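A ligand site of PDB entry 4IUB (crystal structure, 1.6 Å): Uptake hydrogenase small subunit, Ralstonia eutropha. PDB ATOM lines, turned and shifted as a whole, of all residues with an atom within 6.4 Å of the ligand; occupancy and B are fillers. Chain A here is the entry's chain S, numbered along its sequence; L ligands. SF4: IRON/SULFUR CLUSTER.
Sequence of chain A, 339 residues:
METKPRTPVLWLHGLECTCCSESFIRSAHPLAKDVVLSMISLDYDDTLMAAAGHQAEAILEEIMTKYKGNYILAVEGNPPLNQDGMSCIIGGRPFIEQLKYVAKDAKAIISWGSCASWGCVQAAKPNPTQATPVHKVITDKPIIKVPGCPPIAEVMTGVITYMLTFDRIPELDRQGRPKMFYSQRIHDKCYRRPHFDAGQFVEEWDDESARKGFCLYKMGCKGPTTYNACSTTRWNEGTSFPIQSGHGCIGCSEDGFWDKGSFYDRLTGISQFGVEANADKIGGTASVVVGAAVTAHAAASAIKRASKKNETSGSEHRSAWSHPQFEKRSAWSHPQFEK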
ATOM      1  N   ILE A 186      -9.536  -5.721 -31.921  1.00  0.00           N
ATOM      2  CA  ILE A 186      -9.496  -5.517 -30.451  1.00  0.00           C
ATOM      3  C   ILE A 186     -10.877  -5.087 -29.921  1.00  0.00           C
ATOM      4  O   ILE A 186     -11.337  -5.571 -28.878  1.00  0.00           O
ATOM      5  CB  ILE A 186      -8.464  -4.433 -30.049  1.00  0.00           C
ATOM      6  CG1 ILE A 186      -7.077  -4.706 -30.632  1.00  0.00           C
ATOM      7  CG2 ILE A 186      -8.400  -4.274 -28.531  1.00  0.00           C
ATOM      8  CD1 ILE A 186      -6.453  -5.996 -30.161  1.00  0.00           C
ATOM      9  N   HIS A 187     -11.505  -4.181 -30.652  1.00  0.00           N
ATOM     10  CA  HIS A 187     -12.798  -3.583 -30.301  1.00  0.00           C
ATOM     11  C   HIS A 187     -13.949  -4.582 -30.245  1.00  0.00           C
ATOM     12  O   HIS A 187     -14.939  -4.330 -29.561  1.00  0.00           O
ATOM     13  CB  HIS A 187     -13.062  -2.481 -31.330  1.00  0.00           C
ATOM     14  CG  HIS A 187     -14.292  -1.626 -31.072  1.00  0.00           C
ATOM     15  ND1 HIS A 187     -14.319  -0.648 -30.130  1.00  0.00           N
ATOM     16  CD2 HIS A 187     -15.506  -1.548 -31.757  1.00  0.00           C
ATOM     17  CE1 HIS A 187     -15.517  -0.037 -30.171  1.00  0.00           C
ATOM     18  NE2 HIS A 187     -16.237  -0.574 -31.171  1.00  0.00           N
ATOM     19  N   ASP A 188     -13.822  -5.708 -30.945  1.00  0.00           N
ATOM     20  CA  ASP A 188     -14.902  -6.715 -30.995  1.00  0.00           C
ATOM     21  C   ASP A 188     -15.279  -7.246 -29.607  1.00  0.00           C
ATOM     22  O   ASP A 188     -16.461  -7.315 -29.268  1.00  0.00           O
ATOM     23  CB  ASP A 188     -14.529  -7.914 -31.896  1.00  0.00           C
ATOM     24  CG  ASP A 188     -14.491  -7.568 -33.383  1.00  0.00           C
ATOM     25  OD1 ASP A 188     -15.003  -6.505 -33.790  1.00  0.00           O
ATOM     26  OD2 ASP A 188     -13.936  -8.378 -34.162  1.00  0.00           O
ATOM     27  N   CYS A 190     -13.416  -6.283 -26.626  1.00  0.00           N
ATOM     28  CA  CYS A 190     -12.883  -5.399 -25.571  1.00  0.00           C
ATOM     29  C   CYS A 190     -13.903  -5.234 -24.433  1.00  0.00           C
ATOM     30  O   CYS A 190     -15.051  -4.904 -24.691  1.00  0.00           O
ATOM     31  CB  CYS A 190     -12.533  -4.016 -26.128  1.00  0.00           C
ATOM     32  SG  CYS A 190     -11.904  -2.868 -24.876  1.00  0.00           S
ATOM     33  N   TYR A 191     -13.474  -5.451 -23.197  1.00  0.00           N
ATOM     34  CA  TYR A 191     -14.431  -5.438 -22.091  1.00  0.00           C
ATOM     35  C   TYR A 191     -15.014  -4.044 -21.830  1.00  0.00           C
ATOM     36  O   TYR A 191     -16.002  -3.910 -21.122  1.00  0.00           O
ATOM     37  CB  TYR A 191     -13.792  -5.990 -20.796  1.00  0.00           C
ATOM     38  CG  TYR A 191     -12.931  -4.990 -20.089  1.00  0.00           C
ATOM     39  CD1 TYR A 191     -11.641  -4.709 -20.548  1.00  0.00           C
ATOM     40  CD2 TYR A 191     -13.392  -4.299 -18.967  1.00  0.00           C
ATOM     41  CE1 TYR A 191     -10.842  -3.780 -19.897  1.00  0.00           C
ATOM     42  CE2 TYR A 191     -12.605  -3.364 -18.320  1.00  0.00           C
ATOM     43  CZ  TYR A 191     -11.331  -3.109 -18.787  1.00  0.00           C
ATOM     44  OH  TYR A 191     -10.538  -2.183 -18.150  1.00  0.00           O
ATOM     45  N   ARG A 192     -14.400  -3.017 -22.422  1.00  0.00           N
ATOM     46  CA  ARG A 192     -14.918  -1.646 -22.301  1.00  0.00           C
ATOM     47  C   ARG A 192     -15.968  -1.354 -23.370  1.00  0.00           C
ATOM     48  O   ARG A 192     -16.517  -0.253 -23.404  1.00  0.00           O
ATOM     49  CB  ARG A 192     -13.783  -0.604 -22.320  1.00  0.00           C
ATOM     50  CG  ARG A 192     -12.787  -0.769 -21.178  1.00  0.00           C
ATOM     51  CD  ARG A 192     -11.867   0.446 -21.023  1.00  0.00           C
ATOM     52  NE  ARG A 192     -10.901   0.229 -19.941  1.00  0.00           N
ATOM     53  CZ  ARG A 192     -10.255   1.183 -19.262  1.00  0.00           C
ATOM     54  NH1 ARG A 192     -10.465   2.477 -19.533  1.00  0.00           N
ATOM     55  NH2 ARG A 192      -9.407   0.845 -18.308  1.00  0.00           N
ATOM     56  N   ARG A 193     -16.262  -2.334 -24.217  1.00  0.00           N
ATOM     57  CA  ARG A 193     -17.225  -2.156 -25.315  1.00  0.00           C
ATOM     58  C   ARG A 193     -18.620  -1.671 -24.857  1.00  0.00           C
ATOM     59  O   ARG A 193     -19.229  -0.836 -25.529  1.00  0.00           O
ATOM     60  CB  ARG A 193     -17.313  -3.404 -26.200  1.00  0.00           C
ATOM     61  CG  ARG A 193     -18.257  -3.318 -27.395  1.00  0.00           C
ATOM     62  CD  ARG A 193     -17.759  -2.337 -28.446  1.00  0.00           C
ATOM     63  NE  ARG A 193     -18.648  -2.300 -29.599  1.00  0.00           N
ATOM     64  CZ  ARG A 193     -18.592  -3.128 -30.637  1.00  0.00           C
ATOM     65  NH1 ARG A 193     -17.674  -4.093 -30.670  1.00  0.00           N
ATOM     66  NH2 ARG A 193     -19.452  -3.006 -31.641  1.00  0.00           N
ATOM     67  N   PRO A 194     -19.134  -2.191 -23.721  1.00  0.00           N
ATOM     68  CA  PRO A 194     -20.421  -1.661 -23.248  1.00  0.00           C
ATOM     69  C   PRO A 194     -20.396  -0.166 -22.976  1.00  0.00           C
ATOM     70  O   PRO A 194     -21.413   0.516 -23.192  1.00  0.00           O
ATOM     71  CB  PRO A 194     -20.680  -2.447 -21.963  1.00  0.00           C
ATOM     72  CG  PRO A 194     -19.979  -3.740 -22.188  1.00  0.00           C
ATOM     73  CD  PRO A 194     -18.712  -3.364 -22.937  1.00  0.00           C
ATOM     74  N   HIS A 195     -19.263   0.368 -22.515  1.00  0.00           N
ATOM     75  CA  HIS A 195     -19.147   1.818 -22.332  1.00  0.00           C
ATOM     76  C   HIS A 195     -19.141   2.539 -23.653  1.00  0.00           C
ATOM     77  O   HIS A 195     -19.808   3.564 -23.811  1.00  0.00           O
ATOM     78  CB  HIS A 195     -17.928   2.195 -21.497  1.00  0.00           C
ATOM     79  CG  HIS A 195     -18.016   1.706 -20.068  1.00  0.00           C
ATOM     80  ND1 HIS A 195     -19.043   2.004 -19.256  1.00  0.00           N
ATOM     81  CD2 HIS A 195     -17.145   0.911 -19.319  1.00  0.00           C
ATOM     82  CE1 HIS A 195     -18.851   1.433 -18.051  1.00  0.00           C
ATOM     83  NE2 HIS A 195     -17.695   0.762 -18.094  1.00  0.00           N
ATOM     84  N   PHE A 196     -18.402   2.015 -24.618  1.00  0.00           N
ATOM     85  CA  PHE A 196     -18.413   2.574 -25.976  1.00  0.00           C
ATOM     86  C   PHE A 196     -19.842   2.638 -26.509  1.00  0.00           C
ATOM     87  O   PHE A 196     -20.279   3.674 -27.012  1.00  0.00           O
ATOM     88  CB  PHE A 196     -17.512   1.746 -26.914  1.00  0.00           C
ATOM     89  CG  PHE A 196     -17.539   2.199 -28.349  1.00  0.00           C
ATOM     90  CD1 PHE A 196     -18.489   1.693 -29.251  1.00  0.00           C
ATOM     91  CD2 PHE A 196     -16.615   3.121 -28.816  1.00  0.00           C
ATOM     92  CE1 PHE A 196     -18.501   2.100 -30.567  1.00  0.00           C
ATOM     93  CE2 PHE A 196     -16.632   3.547 -30.142  1.00  0.00           C
ATOM     94  CZ  PHE A 196     -17.571   3.025 -31.021  1.00  0.00           C
ATOM     95  N   PHE A 201     -17.164   7.668 -22.202  1.00  0.00           N
ATOM     96  CA  PHE A 201     -15.781   7.850 -22.631  1.00  0.00           C
ATOM     97  C   PHE A 201     -14.955   8.620 -21.617  1.00  0.00           C
ATOM     98  O   PHE A 201     -15.439   9.550 -20.962  1.00  0.00           O
ATOM     99  CB  PHE A 201     -15.730   8.641 -23.952  1.00  0.00           C
ATOM    100  CG  PHE A 201     -16.474   7.999 -25.090  1.00  0.00           C
ATOM    101  CD1 PHE A 201     -15.985   6.840 -25.693  1.00  0.00           C
ATOM    102  CD2 PHE A 201     -17.655   8.564 -25.591  1.00  0.00           C
ATOM    103  CE1 PHE A 201     -16.663   6.239 -26.745  1.00  0.00           C
ATOM    104  CE2 PHE A 201     -18.329   7.982 -26.657  1.00  0.00           C
ATOM    105  CZ  PHE A 201     -17.829   6.808 -27.238  1.00  0.00           C
ATOM    106  N   PHE A 214     -14.024   3.604 -18.295  1.00  0.00           N
ATOM    107  CA  PHE A 214     -14.799   3.981 -19.483  1.00  0.00           C
ATOM    108  C   PHE A 214     -13.958   3.810 -20.758  1.00  0.00           C
ATOM    109  O   PHE A 214     -12.733   3.663 -20.701  1.00  0.00           O
ATOM    110  CB  PHE A 214     -15.319   5.424 -19.365  1.00  0.00           C
ATOM    111  CG  PHE A 214     -16.567   5.557 -18.527  1.00  0.00           C
ATOM    112  CD1 PHE A 214     -17.008   4.508 -17.722  1.00  0.00           C
ATOM    113  CD2 PHE A 214     -17.292   6.747 -18.531  1.00  0.00           C
ATOM    114  CE1 PHE A 214     -18.163   4.638 -16.947  1.00  0.00           C
ATOM    115  CE2 PHE A 214     -18.438   6.877 -17.759  1.00  0.00           C
ATOM    116  CZ  PHE A 214     -18.876   5.825 -16.971  1.00  0.00           C
ATOM    117  N   CYS A 215     -14.623   3.821 -21.909  1.00  0.00           N
ATOM    118  CA  CYS A 215     -13.954   3.571 -23.191  1.00  0.00           C
ATOM    119  C   CYS A 215     -12.924   4.653 -23.509  1.00  0.00           C
ATOM    120  O   CYS A 215     -13.107   5.826 -23.168  1.00  0.00           O
ATOM    121  CB  CYS A 215     -15.006   3.447 -24.292  1.00  0.00           C
ATOM    122  SG  CYS A 215     -14.370   3.518 -25.993  1.00  0.00           S
ATOM    123  N   LEU A 216     -11.842   4.234 -24.170  1.00  0.00           N
ATOM    124  CA  LEU A 216     -10.691   5.098 -24.449  1.00  0.00           C
ATOM    125  C   LEU A 216     -10.661   5.616 -25.881  1.00  0.00           C
ATOM    126  O   LEU A 216      -9.658   6.177 -26.305  1.00  0.00           O
ATOM    127  CB  LEU A 216      -9.383   4.337 -24.146  1.00  0.00           C
ATOM    128  CG  LEU A 216      -9.205   3.953 -22.675  1.00  0.00           C
ATOM    129  CD1 LEU A 216      -8.114   2.908 -22.495  1.00  0.00           C
ATOM    130  CD2 LEU A 216      -8.898   5.183 -21.821  1.00  0.00           C
ATOM    131  N   TYR A 217     -11.766   5.448 -26.619  1.00  0.00           N
ATOM    132  CA  TYR A 217     -11.855   5.934 -27.999  1.00  0.00           C
ATOM    133  C   TYR A 217     -11.438   7.406 -28.175  1.00  0.00           C
ATOM    134  O   TYR A 217     -10.684   7.735 -29.079  1.00  0.00           O
ATOM    135  CB  TYR A 217     -13.280   5.738 -28.528  1.00  0.00           C
ATOM    136  CG  TYR A 217     -13.469   6.111 -29.975  1.00  0.00           C
ATOM    137  CD1 TYR A 217     -13.236   5.180 -30.976  1.00  0.00           C
ATOM    138  CD2 TYR A 217     -13.904   7.374 -30.337  1.00  0.00           C
ATOM    139  CE1 TYR A 217     -13.427   5.496 -32.316  1.00  0.00           C
ATOM    140  CE2 TYR A 217     -14.090   7.707 -31.668  1.00  0.00           C
ATOM    141  CZ  TYR A 217     -13.850   6.766 -32.654  1.00  0.00           C
ATOM    142  OH  TYR A 217     -14.035   7.085 -33.982  1.00  0.00           O
ATOM    143  N   LYS A 218     -11.923   8.274 -27.300  1.00  0.00           N
ATOM    144  CA  LYS A 218     -11.661   9.703 -27.428  1.00  0.00           C
ATOM    145  C   LYS A 218     -10.243  10.087 -27.003  1.00  0.00           C
ATOM    146  O   LYS A 218      -9.801  11.213 -27.244  1.00  0.00           O
ATOM    147  CB  LYS A 218     -12.714  10.512 -26.661  1.00  0.00           C
ATOM    148  CG  LYS A 218     -14.098  10.392 -27.264  1.00  0.00           C
ATOM    149  CD  LYS A 218     -15.067  11.350 -26.595  1.00  0.00           C
ATOM    150  CE  LYS A 218     -16.415  11.336 -27.302  1.00  0.00           C
ATOM    151  NZ  LYS A 218     -17.362  12.301 -26.679  1.00  0.00           N
ATOM    152  N   CYS A 221      -7.773   5.543 -28.762  1.00  0.00           N
ATOM    153  CA  CYS A 221      -7.722   4.083 -28.879  1.00  0.00           C
ATOM    154  C   CYS A 221      -7.933   3.626 -30.316  1.00  0.00           C
ATOM    155  O   CYS A 221      -8.933   3.981 -30.947  1.00  0.00           O
ATOM    156  CB  CYS A 221      -8.777   3.417 -28.002  1.00  0.00           C
ATOM    157  SG  CYS A 221      -8.638   1.607 -27.994  1.00  0.00           S
ATOM    158  N   LYS A 222      -6.995   2.832 -30.819  1.00  0.00           N
ATOM    159  CA  LYS A 222      -7.086   2.344 -32.194  1.00  0.00           C
ATOM    160  C   LYS A 222      -7.635   0.911 -32.238  1.00  0.00           C
ATOM    161  O   LYS A 222      -7.554   0.247 -33.269  1.00  0.00           O
ATOM    162  CB  LYS A 222      -5.734   2.468 -32.909  1.00  0.00           C
ATOM    163  CG  LYS A 222      -5.184   3.891 -32.976  1.00  0.00           C
ATOM    164  CD  LYS A 222      -6.219   4.895 -33.513  1.00  0.00           C
ATOM    165  CE  LYS A 222      -5.632   6.264 -33.820  1.00  0.00           C
ATOM    166  NZ  LYS A 222      -4.973   6.935 -32.672  1.00  0.00           N
ATOM    167  N   GLY A 223      -8.221   0.463 -31.134  1.00  0.00           N
ATOM    168  CA  GLY A 223      -8.843  -0.866 -31.097  1.00  0.00           C
ATOM    169  C   GLY A 223      -9.796  -1.164 -32.249  1.00  0.00           C
ATOM    170  O   GLY A 223      -9.822  -2.281 -32.762  1.00  0.00           O
ATOM    171  N   PRO A 224     -10.619  -0.173 -32.653  1.00  0.00           N
ATOM    172  CA  PRO A 224     -11.607  -0.405 -33.716  1.00  0.00           C
ATOM    173  C   PRO A 224     -11.018  -0.757 -35.092  1.00  0.00           C
ATOM    174  O   PRO A 224     -11.733  -1.292 -35.949  1.00  0.00           O
ATOM    175  CB  PRO A 224     -12.361   0.930 -33.777  1.00  0.00           C
ATOM    176  CG  PRO A 224     -12.304   1.426 -32.379  1.00  0.00           C
ATOM    177  CD  PRO A 224     -10.892   1.097 -31.952  1.00  0.00           C
ATOM    178  N   SER A 231      -7.611  -8.456 -26.535  1.00  0.00           N
ATOM    179  CA  SER A 231      -8.797  -8.335 -25.685  1.00  0.00           C
ATOM    180  C   SER A 231      -9.241  -9.675 -25.116  1.00  0.00           C
ATOM    181  O   SER A 231      -9.948  -9.730 -24.115  1.00  0.00           O
ATOM    182  CB  SER A 231      -9.968  -7.752 -26.480  1.00  0.00           C
ATOM    183  OG  SER A 231      -9.695  -6.436 -26.900  1.00  0.00           O
ATOM    184  N   PHE A 241      -4.179  -6.032 -20.529  1.00  0.00           N
ATOM    185  CA  PHE A 241      -3.784  -5.608 -21.882  1.00  0.00           C
ATOM    186  C   PHE A 241      -3.792  -4.085 -21.901  1.00  0.00           C
ATOM    187  O   PHE A 241      -4.244  -3.471 -20.940  1.00  0.00           O
ATOM    188  CB  PHE A 241      -4.611  -6.257 -23.009  1.00  0.00           C
ATOM    189  CG  PHE A 241      -6.078  -5.842 -23.074  1.00  0.00           C
ATOM    190  CD1 PHE A 241      -6.978  -6.122 -22.038  1.00  0.00           C
ATOM    191  CD2 PHE A 241      -6.570  -5.229 -24.231  1.00  0.00           C
ATOM    192  CE1 PHE A 241      -8.319  -5.788 -22.144  1.00  0.00           C
ATOM    193  CE2 PHE A 241      -7.914  -4.868 -24.343  1.00  0.00           C
ATOM    194  CZ  PHE A 241      -8.786  -5.150 -23.296  1.00  0.00           C
ATOM    195  N   ILE A 243      -5.518  -1.608 -22.975  1.00  0.00           N
ATOM    196  CA  ILE A 243      -6.767  -0.940 -22.624  1.00  0.00           C
ATOM    197  C   ILE A 243      -7.176  -1.174 -21.162  1.00  0.00           C
ATOM    198  O   ILE A 243      -7.570  -0.246 -20.462  1.00  0.00           O
ATOM    199  CB  ILE A 243      -7.881  -1.358 -23.606  1.00  0.00           C
ATOM    200  CG1 ILE A 243      -7.634  -0.683 -24.961  1.00  0.00           C
ATOM    201  CG2 ILE A 243      -9.264  -1.019 -23.059  1.00  0.00           C
ATOM    202  CD1 ILE A 243      -7.975  -1.559 -26.147  1.00  0.00           C
ATOM    203  N   GLY A 248      -5.103   3.699 -24.469  1.00  0.00           N
ATOM    204  CA  GLY A 248      -5.709   3.171 -25.690  1.00  0.00           C
ATOM    205  C   GLY A 248      -4.730   2.307 -26.471  1.00  0.00           C
ATOM    206  O   GLY A 248      -3.511   2.458 -26.379  1.00  0.00           O
ATOM    207  N   CYS A 249      -5.275   1.374 -27.239  1.00  0.00           N
ATOM    208  CA  CYS A 249      -4.473   0.676 -28.237  1.00  0.00           C
ATOM    209  C   CYS A 249      -3.826   1.714 -29.166  1.00  0.00           C
ATOM    210  O   CYS A 249      -4.479   2.681 -29.567  1.00  0.00           O
ATOM    211  CB  CYS A 249      -5.373  -0.294 -29.021  1.00  0.00           C
ATOM    212  SG  CYS A 249      -4.632  -1.123 -30.458  1.00  0.00           S
HETATM  213 FE1  SF4 L   1     -13.097  -0.141 -28.551  1.00  0.00          FE
HETATM  214 FE2  SF4 L   1     -10.781   0.962 -27.524  1.00  0.00          FE
HETATM  215 FE3  SF4 L   1     -12.194  -0.960 -26.104  1.00  0.00          FE
HETATM  216 FE4  SF4 L   1     -13.212   1.598 -26.430  1.00  0.00          FE
HETATM  217  S1  SF4 L   1     -11.388   1.039 -25.292  1.00  0.00           S
HETATM  218  S2  SF4 L   1     -14.340  -0.355 -26.655  1.00  0.00           S
HETATM  219  S3  SF4 L   1     -12.485   2.118 -28.526  1.00  0.00           S
HETATM  220  S4  SF4 L   1     -11.206  -1.199 -28.180  1.00  0.00           S
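FE1 of the ligand is bound by ND1 of His 187 (2.1 Å).
The side-chain sulfur (SG) of Cys 215 binds an iron atom (FE4) of the ligand, 2.3 Å away.
FE2 of the ligand is bound by SG of Cys 221, at 2.3 Å.
SG of Cys 190 binds FE3 of the ligand.
S1 of the ligand lies close to N of Leu 216 (3.4 Å).
The backbone NH (N) of Arg 193 lies close to a sulfur (S2) of the ligand, at 3.7 Å.
The backbone carbonyl oxygen (O) of His 187 lies within hydrogen-bond range of the guanidinium group (NH1) of Arg 193.
The backbone NH (N) of His 187 sits at hydrogen-bond distance from the backbone carbonyl oxygen (O) of Gly 223 (3.3 Å).
The side-chain sulfur (SG) of Cys 215 lies close to the backbone NH (N) of Tyr 217, 3.3 Å away.
The backbone NH (N) of Cys 221 lies within hydrogen-bond range of the backbone carbonyl oxygen (O) of Leu 216 (3.2 Å).
The side-chain sulfur (SG) of Cys 221 lies close to the backbone NH (N) of Gly 223, 3.4 Å away.
The backbone NH of Arg 192 sits close to the side-chain sulfur of Cys 190 (3.5 Å).
NH1 of Arg 192 sits at hydrogen-bond distance from O of Phe 214.
The side-chain hydroxyl of Tyr 191 is in hydrogen-bond range of the guanidinium group of Arg 192 (3.0 Å).
C of Arg 192 touches S2 of the ligand, at 3.8 Å.
Phe 196 touches the ligand (CB to S2, 3.8 Å).
Tyr 217 touches the ligand (CB to S3, 3.7 Å).
Gly 223 touches the ligand.
CD of Pro 224 touches S3 of the ligand, 3.9 Å away.
Ile 243 touches the ligand (CG2 to S1, 3.7 Å).
Hydrophobic or aromatic side chains within 4 Å of the ligand: His 187, Phe 196, Tyr 217, Pro 224 and Ile 243.
The nearest printed residue that does not touch the ligand is Ile 186 (4.2 Å).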
